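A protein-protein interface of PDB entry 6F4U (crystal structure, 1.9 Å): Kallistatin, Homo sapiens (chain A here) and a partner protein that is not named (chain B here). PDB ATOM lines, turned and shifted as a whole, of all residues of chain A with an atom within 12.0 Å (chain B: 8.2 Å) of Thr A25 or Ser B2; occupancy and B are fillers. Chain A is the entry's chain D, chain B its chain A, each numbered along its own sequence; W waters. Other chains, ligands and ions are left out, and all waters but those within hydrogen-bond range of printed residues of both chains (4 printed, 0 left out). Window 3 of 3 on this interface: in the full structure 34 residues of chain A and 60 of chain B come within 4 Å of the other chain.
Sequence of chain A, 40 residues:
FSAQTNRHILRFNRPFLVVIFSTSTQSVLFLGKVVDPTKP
O of Asp B227 sits at hydrogen-bond distance from N of Thr A23, at 3.2 Å.
O of His B77 is in hydrogen-bond range of OG1 of Thr B81.
N of Leu A29 is in hydrogen-bond range of O of Ile A20.
The side-chain hydroxyl (OG) of Ser A22 is in hydrogen-bond range of the side-chain hydroxyl (OG1) of Thr A25, at 2.8 Å.
The backbone NH of Ser A22 lies within hydrogen-bond range of the backbone carbonyl oxygen of Ser A27, at 2.8 Å.
The side-chain amide nitrogen (NE2) of Gln A26 is in hydrogen-bond range of the backbone carbonyl oxygen (O) of Thr A23 (2.9 Å).
The side-chain hydroxyl of Thr A25 sits at hydrogen-bond distance from the side-chain hydroxyl of Ser A27 (2.8 Å).
Among the printed residues, merely in contact across the chains: Phe A21 with Ala B228 (3.2 Å), Thr A25 with Leu B78 (3.2 Å), Ser A27 with Leu B78 (3.3 Å), Ser A22 with Leu B82 (3.5 Å), Thr A25 with Thr B81 (3.6 Å), Ser A22 with Asp B227 (3.6 Å), Leu A29 with Leu B34 (3.7 Å), Gln A26 with Leu B3 (3.7 Å), Val A28 with Leu B34 (3.8 Å), Gln A26 with Ala B6 (3.8 Å), Ser A24 with Thr B81 (3.8 Å), Ser A24 with Asp B227 (3.9 Å), Thr A25 with Ser B2 (3.9 Å), Thr A25 with Leu B3 (3.9 Å), Thr A25 with Leu B82 (3.98 Å) and Leu A29 with Leu B82 (3.99 Å).
Printed residues of chain B within 4 Å of Thr A25: Ser B2, Leu B3, Leu B78, Thr B81 and Leu B82.
Ser B2 touches one residue of chain A.
Ser A24 touches just these residues of chain B: Thr B81 (3.8 Å) and Asp B227 (3.9 Å).
Leu B3 touches two residues of chain A.
No residue of chain A comes within 4 Å of Ile B5.
Of the printed residues of chain A, Leu B78 touches Thr A25 and Ser A27.
Printed residues of chain A within 4 Å of Thr B81: Ser A24 and Thr A25.
Printed residues of chain B within 4 Å of Phe A21: Ala B228 (3.2 Å).
Of the printed residues of chain A, Leu B82 touches Ser A22 (3.5 Å), Thr A25 (3.98 Å) and Leu A29 (3.99 Å).
Of the printed residues of chain B, Ser A22 touches Leu B82 and Asp B227.
Of the printed residues of chain B, Gln A26 touches Leu B3 and Ala B6.
Of the printed residues of chain B, Leu A29 touches Leu B34 (3.7 Å) and Leu B82 (3.99 Å).
His B80 touches none of the printed residues of chain A.
The nearest residue of chain A that does not touch Ser B2 is Ser A24 (4.9 Å).
Of the 12 printed residues of chain A, 9 touch a printed residue of chain B.
Along chain A the printed residues that touch a printed residue of chain B span positions 21 to 29.
Of the 25 printed residues of chain B, 9 touch a printed residue of chain A.
Hydrophobic or aromatic side chains of chain B that line the printed part of chain A: Leu B3, Ala B6, Leu B34, Leu B78, Leu B82 and Ala B228.
Among the printed residues, 17 pairs touch across the chains.
Water W4 lies within hydrogen-bond range of the backbone carbonyl oxygen (O) of Ala B6 (2.6 Å) and the backbone carbonyl oxygen (O) of Gln A26 (2.7 Å).
Water W1 lies within hydrogen-bond range of O of Ser B2 (2.6 Å) and O of Thr A25 (2.6 Å).
Water W2 bridges OG of Ser A27 and ND2 of Asn B9.
Water W3 lies within hydrogen-bond range of the side-chain hydroxyl (OG) of Ser A22 and the backbone carbonyl oxygen (O) of Asp B227.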
ATOM      1  N   VAL A  19     -26.351 -20.792   9.185  1.00  0.00           N
ATOM      2  CA  VAL A  19     -25.597 -20.657  10.445  1.00  0.00           C
ATOM      3  C   VAL A  19     -26.581 -20.879  11.606  1.00  0.00           C
ATOM      4  O   VAL A  19     -27.408 -20.026  11.884  1.00  0.00           O
ATOM      5  CB  VAL A  19     -24.920 -19.275  10.584  1.00  0.00           C
ATOM      6  CG1 VAL A  19     -23.952 -19.274  11.767  1.00  0.00           C
ATOM      7  CG2 VAL A  19     -24.177 -18.905   9.311  1.00  0.00           C
ATOM      8  N   ILE A  20     -26.503 -22.028  12.258  1.00  0.00           N
ATOM      9  CA  ILE A  20     -27.337 -22.284  13.447  1.00  0.00           C
ATOM     10  C   ILE A  20     -26.525 -21.900  14.683  1.00  0.00           C
ATOM     11  O   ILE A  20     -25.439 -22.427  14.902  1.00  0.00           O
ATOM     12  CB  ILE A  20     -27.804 -23.739  13.511  1.00  0.00           C
ATOM     13  CG1 ILE A  20     -28.630 -24.071  12.267  1.00  0.00           C
ATOM     14  CG2 ILE A  20     -28.563 -23.997  14.824  1.00  0.00           C
ATOM     15  CD1 ILE A  20     -29.040 -25.531  12.180  1.00  0.00           C
ATOM     16  N   PHE A  21     -27.103 -21.021  15.496  1.00  0.00           N
ATOM     17  CA  PHE A  21     -26.404 -20.290  16.534  1.00  0.00           C
ATOM     18  C   PHE A  21     -27.119 -20.418  17.878  1.00  0.00           C
ATOM     19  O   PHE A  21     -28.338 -20.203  17.934  1.00  0.00           O
ATOM     20  CB  PHE A  21     -26.355 -18.828  16.063  1.00  0.00           C
ATOM     21  CG  PHE A  21     -25.468 -17.948  16.883  1.00  0.00           C
ATOM     22  CD1 PHE A  21     -26.021 -16.923  17.670  1.00  0.00           C
ATOM     23  CD2 PHE A  21     -24.081 -18.127  16.882  1.00  0.00           C
ATOM     24  CE1 PHE A  21     -25.191 -16.075  18.424  1.00  0.00           C
ATOM     25  CE2 PHE A  21     -23.262 -17.292  17.640  1.00  0.00           C
ATOM     26  CZ  PHE A  21     -23.823 -16.267  18.411  1.00  0.00           C
ATOM     27  N   SER A  22     -26.398 -20.845  18.926  1.00  0.00           N
ATOM     28  CA  SER A  22     -26.905 -20.845  20.293  1.00  0.00           C
ATOM     29  C   SER A  22     -26.757 -19.440  20.848  1.00  0.00           C
ATOM     30  O   SER A  22     -25.646 -18.915  20.964  1.00  0.00           O
ATOM     31  CB  SER A  22     -26.172 -21.865  21.183  1.00  0.00           C
ATOM     32  OG  SER A  22     -26.424 -21.626  22.563  1.00  0.00           O
ATOM     33  N   THR A  23     -27.878 -18.801  21.181  1.00  0.00           N
ATOM     34  CA  THR A  23     -27.808 -17.463  21.721  1.00  0.00           C
ATOM     35  C   THR A  23     -27.403 -17.465  23.207  1.00  0.00           C
ATOM     36  O   THR A  23     -26.821 -16.497  23.643  1.00  0.00           O
ATOM     37  CB  THR A  23     -29.106 -16.644  21.549  1.00  0.00           C
ATOM     38  OG1 THR A  23     -30.155 -17.299  22.236  1.00  0.00           O
ATOM     39  CG2 THR A  23     -29.477 -16.506  20.087  1.00  0.00           C
ATOM     40  N   SER A  24     -27.680 -18.521  23.959  1.00  0.00           N
ATOM     41  CA  SER A  24     -27.251 -18.584  25.365  1.00  0.00           C
ATOM     42  C   SER A  24     -25.740 -18.783  25.505  1.00  0.00           C
ATOM     43  O   SER A  24     -25.153 -18.316  26.457  1.00  0.00           O
ATOM     44  CB  SER A  24     -27.946 -19.703  26.108  1.00  0.00           C
ATOM     45  OG  SER A  24     -27.797 -20.934  25.434  1.00  0.00           O
ATOM     46  N   THR A  25     -25.120 -19.508  24.584  1.00  0.00           N
ATOM     47  CA  THR A  25     -23.691 -19.734  24.657  1.00  0.00           C
ATOM     48  C   THR A  25     -22.863 -18.992  23.621  1.00  0.00           C
ATOM     49  O   THR A  25     -21.620 -19.069  23.657  1.00  0.00           O
ATOM     50  CB  THR A  25     -23.401 -21.224  24.565  1.00  0.00           C
ATOM     51  OG1 THR A  25     -23.680 -21.710  23.245  1.00  0.00           O
ATOM     52  CG2 THR A  25     -24.230 -21.975  25.581  1.00  0.00           C
ATOM     53  N   GLN A  26     -23.529 -18.281  22.703  1.00  0.00           N
ATOM     54  CA  GLN A  26     -22.874 -17.588  21.610  1.00  0.00           C
ATOM     55  C   GLN A  26     -21.990 -18.524  20.750  1.00  0.00           C
ATOM     56  O   GLN A  26     -20.890 -18.148  20.340  1.00  0.00           O
ATOM     57  CB  GLN A  26     -22.087 -16.389  22.148  1.00  0.00           C
ATOM     58  CG  GLN A  26     -22.962 -15.386  22.879  1.00  0.00           C
ATOM     59  CD  GLN A  26     -23.838 -14.610  21.915  1.00  0.00           C
ATOM     60  OE1 GLN A  26     -23.328 -13.887  21.075  1.00  0.00           O
ATOM     61  NE2 GLN A  26     -25.161 -14.765  22.024  1.00  0.00           N
ATOM     62  N   SER A  27     -22.486 -19.735  20.507  1.00  0.00           N
ATOM     63  CA  SER A  27     -21.801 -20.766  19.744  1.00  0.00           C
ATOM     64  C   SER A  27     -22.465 -21.039  18.414  1.00  0.00           C
ATOM     65  O   SER A  27     -23.700 -21.159  18.325  1.00  0.00           O
ATOM     66  CB  SER A  27     -21.797 -22.104  20.499  1.00  0.00           C
ATOM     67  OG  SER A  27     -21.305 -21.918  21.792  1.00  0.00           O
ATOM     68  N   VAL A  28     -21.634 -21.195  17.395  1.00  0.00           N
ATOM     69  CA  VAL A  28     -22.066 -21.740  16.118  1.00  0.00           C
ATOM     70  C   VAL A  28     -22.182 -23.249  16.305  1.00  0.00           C
ATOM     71  O   VAL A  28     -21.189 -23.958  16.416  1.00  0.00           O
ATOM     72  CB  VAL A  28     -21.119 -21.389  14.961  1.00  0.00           C
ATOM     73  CG1 VAL A  28     -21.650 -21.987  13.664  1.00  0.00           C
ATOM     74  CG2 VAL A  28     -21.001 -19.872  14.797  1.00  0.00           C
ATOM     75  N   LEU A  29     -23.421 -23.738  16.361  1.00  0.00           N
ATOM     76  CA  LEU A  29     -23.684 -25.155  16.517  1.00  0.00           C
ATOM     77  C   LEU A  29     -23.505 -25.908  15.212  1.00  0.00           C
ATOM     78  O   LEU A  29     -22.982 -27.038  15.187  1.00  0.00           O
ATOM     79  CB  LEU A  29     -25.106 -25.377  17.068  1.00  0.00           C
ATOM     80  CG  LEU A  29     -25.463 -24.718  18.389  1.00  0.00           C
ATOM     81  CD1 LEU A  29     -26.904 -25.048  18.774  1.00  0.00           C
ATOM     82  CD2 LEU A  29     -24.510 -25.108  19.524  1.00  0.00           C
ATOM     83  N   PHE A  30     -23.909 -25.289  14.112  1.00  0.00           N
ATOM     84  CA  PHE A  30     -23.845 -25.918  12.788  1.00  0.00           C
ATOM     85  C   PHE A  30     -23.638 -24.836  11.757  1.00  0.00           C
ATOM     86  O   PHE A  30     -24.106 -23.707  11.913  1.00  0.00           O
ATOM     87  CB  PHE A  30     -25.147 -26.666  12.438  1.00  0.00           C
ATOM     88  CG  PHE A  30     -25.531 -27.742  13.401  1.00  0.00           C
ATOM     89  CD1 PHE A  30     -25.087 -29.047  13.232  1.00  0.00           C
ATOM     90  CD2 PHE A  30     -26.384 -27.468  14.471  1.00  0.00           C
ATOM     91  CE1 PHE A  30     -25.462 -30.043  14.121  1.00  0.00           C
ATOM     92  CE2 PHE A  30     -26.728 -28.455  15.385  1.00  0.00           C
ATOM     93  CZ  PHE A  30     -26.290 -29.747  15.200  1.00  0.00           C
ATOM     94  N   SER B   2     -19.063 -19.610  29.771  1.00  0.00           N
ATOM     95  CA  SER B   2     -18.606 -20.124  28.429  1.00  0.00           C
ATOM     96  C   SER B   2     -18.262 -19.028  27.407  1.00  0.00           C
ATOM     97  O   SER B   2     -17.779 -19.339  26.306  1.00  0.00           O
ATOM     98  CB  SER B   2     -19.639 -21.089  27.822  1.00  0.00           C
ATOM     99  OG  SER B   2     -20.860 -20.459  27.410  1.00  0.00           O
ATOM    100  N   LEU B   3     -18.458 -17.753  27.771  1.00  0.00           N
ATOM    101  CA  LEU B   3     -18.199 -16.658  26.832  1.00  0.00           C
ATOM    102  C   LEU B   3     -16.720 -16.428  26.541  1.00  0.00           C
ATOM    103  O   LEU B   3     -16.408 -15.925  25.460  1.00  0.00           O
ATOM    104  CB  LEU B   3     -18.911 -15.372  27.252  1.00  0.00           C
ATOM    105  CG  LEU B   3     -20.435 -15.559  27.334  1.00  0.00           C
ATOM    106  CD1 LEU B   3     -21.088 -14.275  27.846  1.00  0.00           C
ATOM    107  CD2 LEU B   3     -21.065 -16.005  26.017  1.00  0.00           C
ATOM    108  N   LYS B   4     -15.817 -16.837  27.436  1.00  0.00           N
ATOM    109  CA  LYS B   4     -14.383 -16.718  27.155  1.00  0.00           C
ATOM    110  C   LYS B   4     -13.919 -17.547  25.948  1.00  0.00           C
ATOM    111  O   LYS B   4     -12.965 -17.167  25.265  1.00  0.00           O
ATOM    112  CB  LYS B   4     -13.514 -17.091  28.375  1.00  0.00           C
ATOM    113  CG  LYS B   4     -13.468 -16.013  29.458  1.00  0.00           C
ATOM    114  CD  LYS B   4     -12.343 -16.281  30.462  1.00  0.00           C
ATOM    115  CE  LYS B   4     -12.264 -15.178  31.505  1.00  0.00           C
ATOM    116  NZ  LYS B   4     -11.244 -15.506  32.539  1.00  0.00           N
ATOM    117  N   ILE B   5     -14.569 -18.681  25.700  1.00  0.00           N
ATOM    118  CA  ILE B   5     -14.176 -19.544  24.564  1.00  0.00           C
ATOM    119  C   ILE B   5     -14.933 -19.243  23.274  1.00  0.00           C
ATOM    120  O   ILE B   5     -14.626 -19.807  22.248  1.00  0.00           O
ATOM    121  CB  ILE B   5     -14.258 -21.048  24.918  1.00  0.00           C
ATOM    122  CG1 ILE B   5     -15.671 -21.516  25.221  1.00  0.00           C
ATOM    123  CG2 ILE B   5     -13.350 -21.313  26.109  1.00  0.00           C
ATOM    124  CD1 ILE B   5     -15.772 -23.023  25.237  1.00  0.00           C
ATOM    125  N   ALA B   6     -15.909 -18.348  23.329  1.00  0.00           N
ATOM    126  CA  ALA B   6     -16.784 -18.101  22.187  1.00  0.00           C
ATOM    127  C   ALA B   6     -15.995 -17.550  20.977  1.00  0.00           C
ATOM    128  O   ALA B   6     -16.196 -18.015  19.876  1.00  0.00           O
ATOM    129  CB  ALA B   6     -17.949 -17.193  22.588  1.00  0.00           C
ATOM    130  N   PRO B   7     -15.038 -16.609  21.185  1.00  0.00           N
ATOM    131  CA  PRO B   7     -14.293 -16.104  20.026  1.00  0.00           C
ATOM    132  C   PRO B   7     -13.486 -17.197  19.290  1.00  0.00           C
ATOM    133  O   PRO B   7     -13.563 -17.299  18.033  1.00  0.00           O
ATOM    134  CB  PRO B   7     -13.332 -15.049  20.655  1.00  0.00           C
ATOM    135  CG  PRO B   7     -14.100 -14.540  21.836  1.00  0.00           C
ATOM    136  CD  PRO B   7     -14.823 -15.759  22.377  1.00  0.00           C
ATOM    137  N   ALA B   8     -12.769 -18.029  20.048  1.00  0.00           N
ATOM    138  CA  ALA B   8     -11.976 -19.137  19.434  1.00  0.00           C
ATOM    139  C   ALA B   8     -12.868 -20.149  18.706  1.00  0.00           C
ATOM    140  O   ALA B   8     -12.578 -20.551  17.567  1.00  0.00           O
ATOM    141  CB  ALA B   8     -11.121 -19.855  20.466  1.00  0.00           C
ATOM    142  N   ASN B   9     -13.950 -20.565  19.349  1.00  0.00           N
ATOM    143  CA  ASN B   9     -14.856 -21.513  18.716  1.00  0.00           C
ATOM    144  C   ASN B   9     -15.424 -20.978  17.380  1.00  0.00           C
ATOM    145  O   ASN B   9     -15.477 -21.718  16.415  1.00  0.00           O
ATOM    146  CB  ASN B   9     -15.983 -21.930  19.668  1.00  0.00           C
ATOM    147  CG  ASN B   9     -15.506 -22.879  20.769  1.00  0.00           C
ATOM    148  OD1 ASN B   9     -14.390 -23.440  20.703  1.00  0.00           O
ATOM    149  ND2 ASN B   9     -16.348 -23.068  21.783  1.00  0.00           N
ATOM    150  N   LEU B  34     -18.890 -26.946  16.736  1.00  0.00           N
ATOM    151  CA  LEU B  34     -18.871 -27.163  18.189  1.00  0.00           C
ATOM    152  C   LEU B  34     -18.499 -28.596  18.520  1.00  0.00           C
ATOM    153  O   LEU B  34     -17.687 -28.834  19.408  1.00  0.00           O
ATOM    154  CB  LEU B  34     -20.240 -26.821  18.805  1.00  0.00           C
ATOM    155  CG  LEU B  34     -20.281 -27.050  20.332  1.00  0.00           C
ATOM    156  CD1 LEU B  34     -19.254 -26.163  20.997  1.00  0.00           C
ATOM    157  CD2 LEU B  34     -21.639 -26.869  20.939  1.00  0.00           C
ATOM    158  N   PHE B  61      -7.534 -20.982  20.155  1.00  0.00           N
ATOM    159  CA  PHE B  61      -7.345 -20.423  21.494  1.00  0.00           C
ATOM    160  C   PHE B  61      -6.023 -19.659  21.588  1.00  0.00           C
ATOM    161  O   PHE B  61      -4.998 -20.143  21.116  1.00  0.00           O
ATOM    162  CB  PHE B  61      -7.465 -21.495  22.564  1.00  0.00           C
ATOM    163  CG  PHE B  61      -8.842 -22.051  22.653  1.00  0.00           C
ATOM    164  CD1 PHE B  61      -9.863 -21.274  23.172  1.00  0.00           C
ATOM    165  CD2 PHE B  61      -9.139 -23.295  22.157  1.00  0.00           C
ATOM    166  CE1 PHE B  61     -11.153 -21.750  23.228  1.00  0.00           C
ATOM    167  CE2 PHE B  61     -10.449 -23.775  22.190  1.00  0.00           C
ATOM    168  CZ  PHE B  61     -11.455 -22.991  22.722  1.00  0.00           C
ATOM    169  N   ASP B  70      -9.176 -22.126  31.732  1.00  0.00           N
ATOM    170  CA  ASP B  70     -10.250 -21.302  31.192  1.00  0.00           C
ATOM    171  C   ASP B  70     -10.934 -22.021  29.992  1.00  0.00           C
ATOM    172  O   ASP B  70     -12.142 -21.904  29.809  1.00  0.00           O
ATOM    173  CB  ASP B  70      -9.737 -19.945  30.660  1.00  0.00           C
ATOM    174  CG  ASP B  70      -9.306 -18.955  31.758  1.00  0.00           C
ATOM    175  OD1 ASP B  70      -9.977 -18.831  32.806  1.00  0.00           O
ATOM    176  OD2 ASP B  70      -8.290 -18.254  31.503  1.00  0.00           O
ATOM    177  N   VAL B  71     -10.156 -22.710  29.173  1.00  0.00           N
ATOM    178  CA  VAL B  71     -10.701 -23.403  27.977  1.00  0.00           C
ATOM    179  C   VAL B  71     -11.574 -24.577  28.404  1.00  0.00           C
ATOM    180  O   VAL B  71     -12.720 -24.688  27.973  1.00  0.00           O
ATOM    181  CB  VAL B  71      -9.577 -23.900  27.046  1.00  0.00           C
ATOM    182  CG1 VAL B  71     -10.114 -24.787  25.936  1.00  0.00           C
ATOM    183  CG2 VAL B  71      -8.754 -22.715  26.486  1.00  0.00           C
ATOM    184  N   ARG B  73     -12.893 -25.457  31.472  1.00  0.00           N
ATOM    185  CA  ARG B  73     -14.039 -25.018  32.236  1.00  0.00           C
ATOM    186  C   ARG B  73     -15.058 -24.247  31.367  1.00  0.00           C
ATOM    187  O   ARG B  73     -16.273 -24.332  31.605  1.00  0.00           O
ATOM    188  CB  ARG B  73     -13.606 -24.185  33.444  1.00  0.00           C
ATOM    189  CG  ARG B  73     -12.672 -24.922  34.413  1.00  0.00           C
ATOM    190  CD  ARG B  73     -13.253 -26.256  34.880  1.00  0.00           C
ATOM    191  NE  ARG B  73     -12.339 -26.993  35.745  1.00  0.00           N
ATOM    192  CZ  ARG B  73     -12.628 -28.154  36.347  1.00  0.00           C
ATOM    193  NH1 ARG B  73     -13.824 -28.734  36.184  1.00  0.00           N
ATOM    194  NH2 ARG B  73     -11.716 -28.732  37.124  1.00  0.00           N
ATOM    195  N   GLY B  74     -14.569 -23.517  30.369  1.00  0.00           N
ATOM    196  CA  GLY B  74     -15.449 -22.907  29.369  1.00  0.00           C
ATOM    197  C   GLY B  74     -16.281 -23.960  28.657  1.00  0.00           C
ATOM    198  O   GLY B  74     -17.502 -23.824  28.544  1.00  0.00           O
ATOM    199  N   PHE B  75     -15.646 -25.021  28.189  1.00  0.00           N
ATOM    200  CA  PHE B  75     -16.392 -26.113  27.522  1.00  0.00           C
ATOM    201  C   PHE B  75     -17.344 -26.777  28.489  1.00  0.00           C
ATOM    202  O   PHE B  75     -18.483 -27.077  28.120  1.00  0.00           O
ATOM    203  CB  PHE B  75     -15.477 -27.164  26.891  1.00  0.00           C
ATOM    204  CG  PHE B  75     -14.999 -26.790  25.515  1.00  0.00           C
ATOM    205  CD1 PHE B  75     -15.880 -26.864  24.399  1.00  0.00           C
ATOM    206  CD2 PHE B  75     -13.741 -26.318  25.315  1.00  0.00           C
ATOM    207  CE1 PHE B  75     -15.448 -26.512  23.144  1.00  0.00           C
ATOM    208  CE2 PHE B  75     -13.303 -25.960  24.061  1.00  0.00           C
ATOM    209  CZ  PHE B  75     -14.153 -26.062  22.973  1.00  0.00           C
ATOM    210  N   GLN B  76     -16.889 -27.008  29.728  1.00  0.00           N
ATOM    211  CA  GLN B  76     -17.763 -27.644  30.726  1.00  0.00           C
ATOM    212  C   GLN B  76     -19.040 -26.856  30.915  1.00  0.00           C
ATOM    213  O   GLN B  76     -20.115 -27.442  30.923  1.00  0.00           O
ATOM    214  CB  GLN B  76     -17.060 -27.785  32.084  1.00  0.00           C
ATOM    215  CG  GLN B  76     -17.904 -28.487  33.145  1.00  0.00           C
ATOM    216  CD  GLN B  76     -17.203 -28.529  34.494  1.00  0.00           C
ATOM    217  OE1 GLN B  76     -16.046 -28.134  34.630  1.00  0.00           O
ATOM    218  NE2 GLN B  76     -17.888 -29.028  35.477  1.00  0.00           N
ATOM    219  N   HIS B  77     -18.921 -25.537  31.051  1.00  0.00           N
ATOM    220  CA  HIS B  77     -20.099 -24.677  31.217  1.00  0.00           C
ATOM    221  C   HIS B  77     -20.949 -24.607  29.945  1.00  0.00           C
ATOM    222  O   HIS B  77     -22.164 -24.585  30.020  1.00  0.00           O
ATOM    223  CB  HIS B  77     -19.709 -23.253  31.641  1.00  0.00           C
ATOM    224  CG  HIS B  77     -20.884 -22.341  31.838  1.00  0.00           C
ATOM    225  ND1 HIS B  77     -21.287 -21.426  30.885  1.00  0.00           N
ATOM    226  CD2 HIS B  77     -21.763 -22.226  32.862  1.00  0.00           C
ATOM    227  CE1 HIS B  77     -22.348 -20.774  31.325  1.00  0.00           C
ATOM    228  NE2 HIS B  77     -22.662 -21.245  32.518  1.00  0.00           N
ATOM    229  N   LEU B  78     -20.296 -24.526  28.785  1.00  0.00           N
ATOM    230  CA  LEU B  78     -21.010 -24.491  27.477  1.00  0.00           C
ATOM    231  C   LEU B  78     -21.870 -25.729  27.325  1.00  0.00           C
ATOM    232  O   LEU B  78     -23.068 -25.632  27.071  1.00  0.00           O
ATOM    233  CB  LEU B  78     -19.999 -24.403  26.346  1.00  0.00           C
ATOM    234  CG  LEU B  78     -20.313 -24.550  24.837  1.00  0.00           C
ATOM    235  CD1 LEU B  78     -21.538 -23.871  24.465  1.00  0.00           C
ATOM    236  CD2 LEU B  78     -19.170 -23.951  24.029  1.00  0.00           C
ATOM    237  N   LEU B  79     -21.267 -26.890  27.533  1.00  0.00           N
ATOM    238  CA  LEU B  79     -21.971 -28.159  27.355  1.00  0.00           C
ATOM    239  C   LEU B  79     -23.086 -28.371  28.385  1.00  0.00           C
ATOM    240  O   LEU B  79     -24.191 -28.821  28.041  1.00  0.00           O
ATOM    241  CB  LEU B  79     -20.973 -29.314  27.356  1.00  0.00           C
ATOM    242  CG  LEU B  79     -19.925 -29.190  26.229  1.00  0.00           C
ATOM    243  CD1 LEU B  79     -18.787 -30.172  26.446  1.00  0.00           C
ATOM    244  CD2 LEU B  79     -20.536 -29.381  24.860  1.00  0.00           C
ATOM    245  N   HIS B  80     -22.816 -28.011  29.634  1.00  0.00           N
ATOM    246  CA  HIS B  80     -23.848 -28.049  30.678  1.00  0.00           C
ATOM    247  C   HIS B  80     -25.048 -27.183  30.290  1.00  0.00           C
ATOM    248  O   HIS B  80     -26.187 -27.644  30.373  1.00  0.00           O
ATOM    249  CB  HIS B  80     -23.269 -27.592  32.026  1.00  0.00           C
ATOM    250  CG  HIS B  80     -24.294 -27.475  33.121  1.00  0.00           C
ATOM    251  ND1 HIS B  80     -24.637 -28.533  33.939  1.00  0.00           N
ATOM    252  CD2 HIS B  80     -25.051 -26.425  33.527  1.00  0.00           C
ATOM    253  CE1 HIS B  80     -25.561 -28.138  34.799  1.00  0.00           C
ATOM    254  NE2 HIS B  80     -25.829 -26.866  34.570  1.00  0.00           N
ATOM    255  N   THR B  81     -24.789 -25.945  29.861  1.00  0.00           N
ATOM    256  CA  THR B  81     -25.823 -25.001  29.449  1.00  0.00           C
ATOM    257  C   THR B  81     -26.664 -25.571  28.284  1.00  0.00           C
ATOM    258  O   THR B  81     -27.916 -25.567  28.342  1.00  0.00           O
ATOM    259  CB  THR B  81     -25.221 -23.633  29.070  1.00  0.00           C
ATOM    260  OG1 THR B  81     -24.606 -23.036  30.222  1.00  0.00           O
ATOM    261  CG2 THR B  81     -26.274 -22.652  28.502  1.00  0.00           C
ATOM    262  N   LEU B  82     -25.994 -26.108  27.250  1.00  0.00           N
ATOM    263  CA  LEU B  82     -26.743 -26.702  26.123  1.00  0.00           C
ATOM    264  C   LEU B  82     -27.628 -27.881  26.534  1.00  0.00           C
ATOM    265  O   LEU B  82     -28.711 -28.070  25.981  1.00  0.00           O
ATOM    266  CB  LEU B  82     -25.797 -27.130  24.984  1.00  0.00           C
ATOM    267  CG  LEU B  82     -25.068 -25.994  24.286  1.00  0.00           C
ATOM    268  CD1 LEU B  82     -24.110 -26.544  23.227  1.00  0.00           C
ATOM    269  CD2 LEU B  82     -26.039 -24.967  23.674  1.00  0.00           C
ATOM    270  N   ASN B  83     -27.178 -28.656  27.508  1.00  0.00           N
ATOM    271  CA  ASN B  83     -27.928 -29.816  27.941  1.00  0.00           C
ATOM    272  C   ASN B  83     -29.084 -29.487  28.887  1.00  0.00           C
ATOM    273  O   ASN B  83     -29.844 -30.372  29.202  1.00  0.00           O
ATOM    274  CB  ASN B  83     -26.988 -30.859  28.581  1.00  0.00           C
ATOM    275  CG  ASN B  83     -26.169 -31.604  27.538  1.00  0.00           C
ATOM    276  OD1 ASN B  83     -26.689 -31.938  26.495  1.00  0.00           O
ATOM    277  ND2 ASN B  83     -24.902 -31.859  27.817  1.00  0.00           N
ATOM    278  N   ASP B 227     -33.288 -21.005  23.028  1.00  0.00           N
ATOM    279  CA  ASP B 227     -32.209 -20.047  22.912  1.00  0.00           C
ATOM    280  C   ASP B 227     -31.349 -20.454  21.709  1.00  0.00           C
ATOM    281  O   ASP B 227     -30.183 -20.849  21.888  1.00  0.00           O
ATOM    282  CB  ASP B 227     -31.368 -20.042  24.194  1.00  0.00           C
ATOM    283  CG  ASP B 227     -32.190 -19.654  25.444  1.00  0.00           C
ATOM    284  OD1 ASP B 227     -33.134 -18.844  25.342  1.00  0.00           O
ATOM    285  OD2 ASP B 227     -31.866 -20.171  26.535  1.00  0.00           O
ATOM    286  N   ALA B 228     -31.948 -20.441  20.525  1.00  0.00           N
ATOM    287  CA  ALA B 228     -31.241 -20.687  19.277  1.00  0.00           C
ATOM    288  C   ALA B 228     -31.873 -19.886  18.165  1.00  0.00           C
ATOM    289  O   ALA B 228     -33.069 -19.562  18.202  1.00  0.00           O
ATOM    290  CB  ALA B 228     -31.229 -22.161  18.930  1.00  0.00           C
HETATM  291  O   HOH W   1     -19.260 -20.107  24.262  1.00  0.00           O
HETATM  292  O   HOH W   2     -18.719 -21.264  21.810  1.00  0.00           O
HETATM  293  O   HOH W   3     -28.730 -23.055  22.582  1.00  0.00           O
HETATM  294  O   HOH W   4     -18.509 -19.233  19.674  1.00  0.00           O
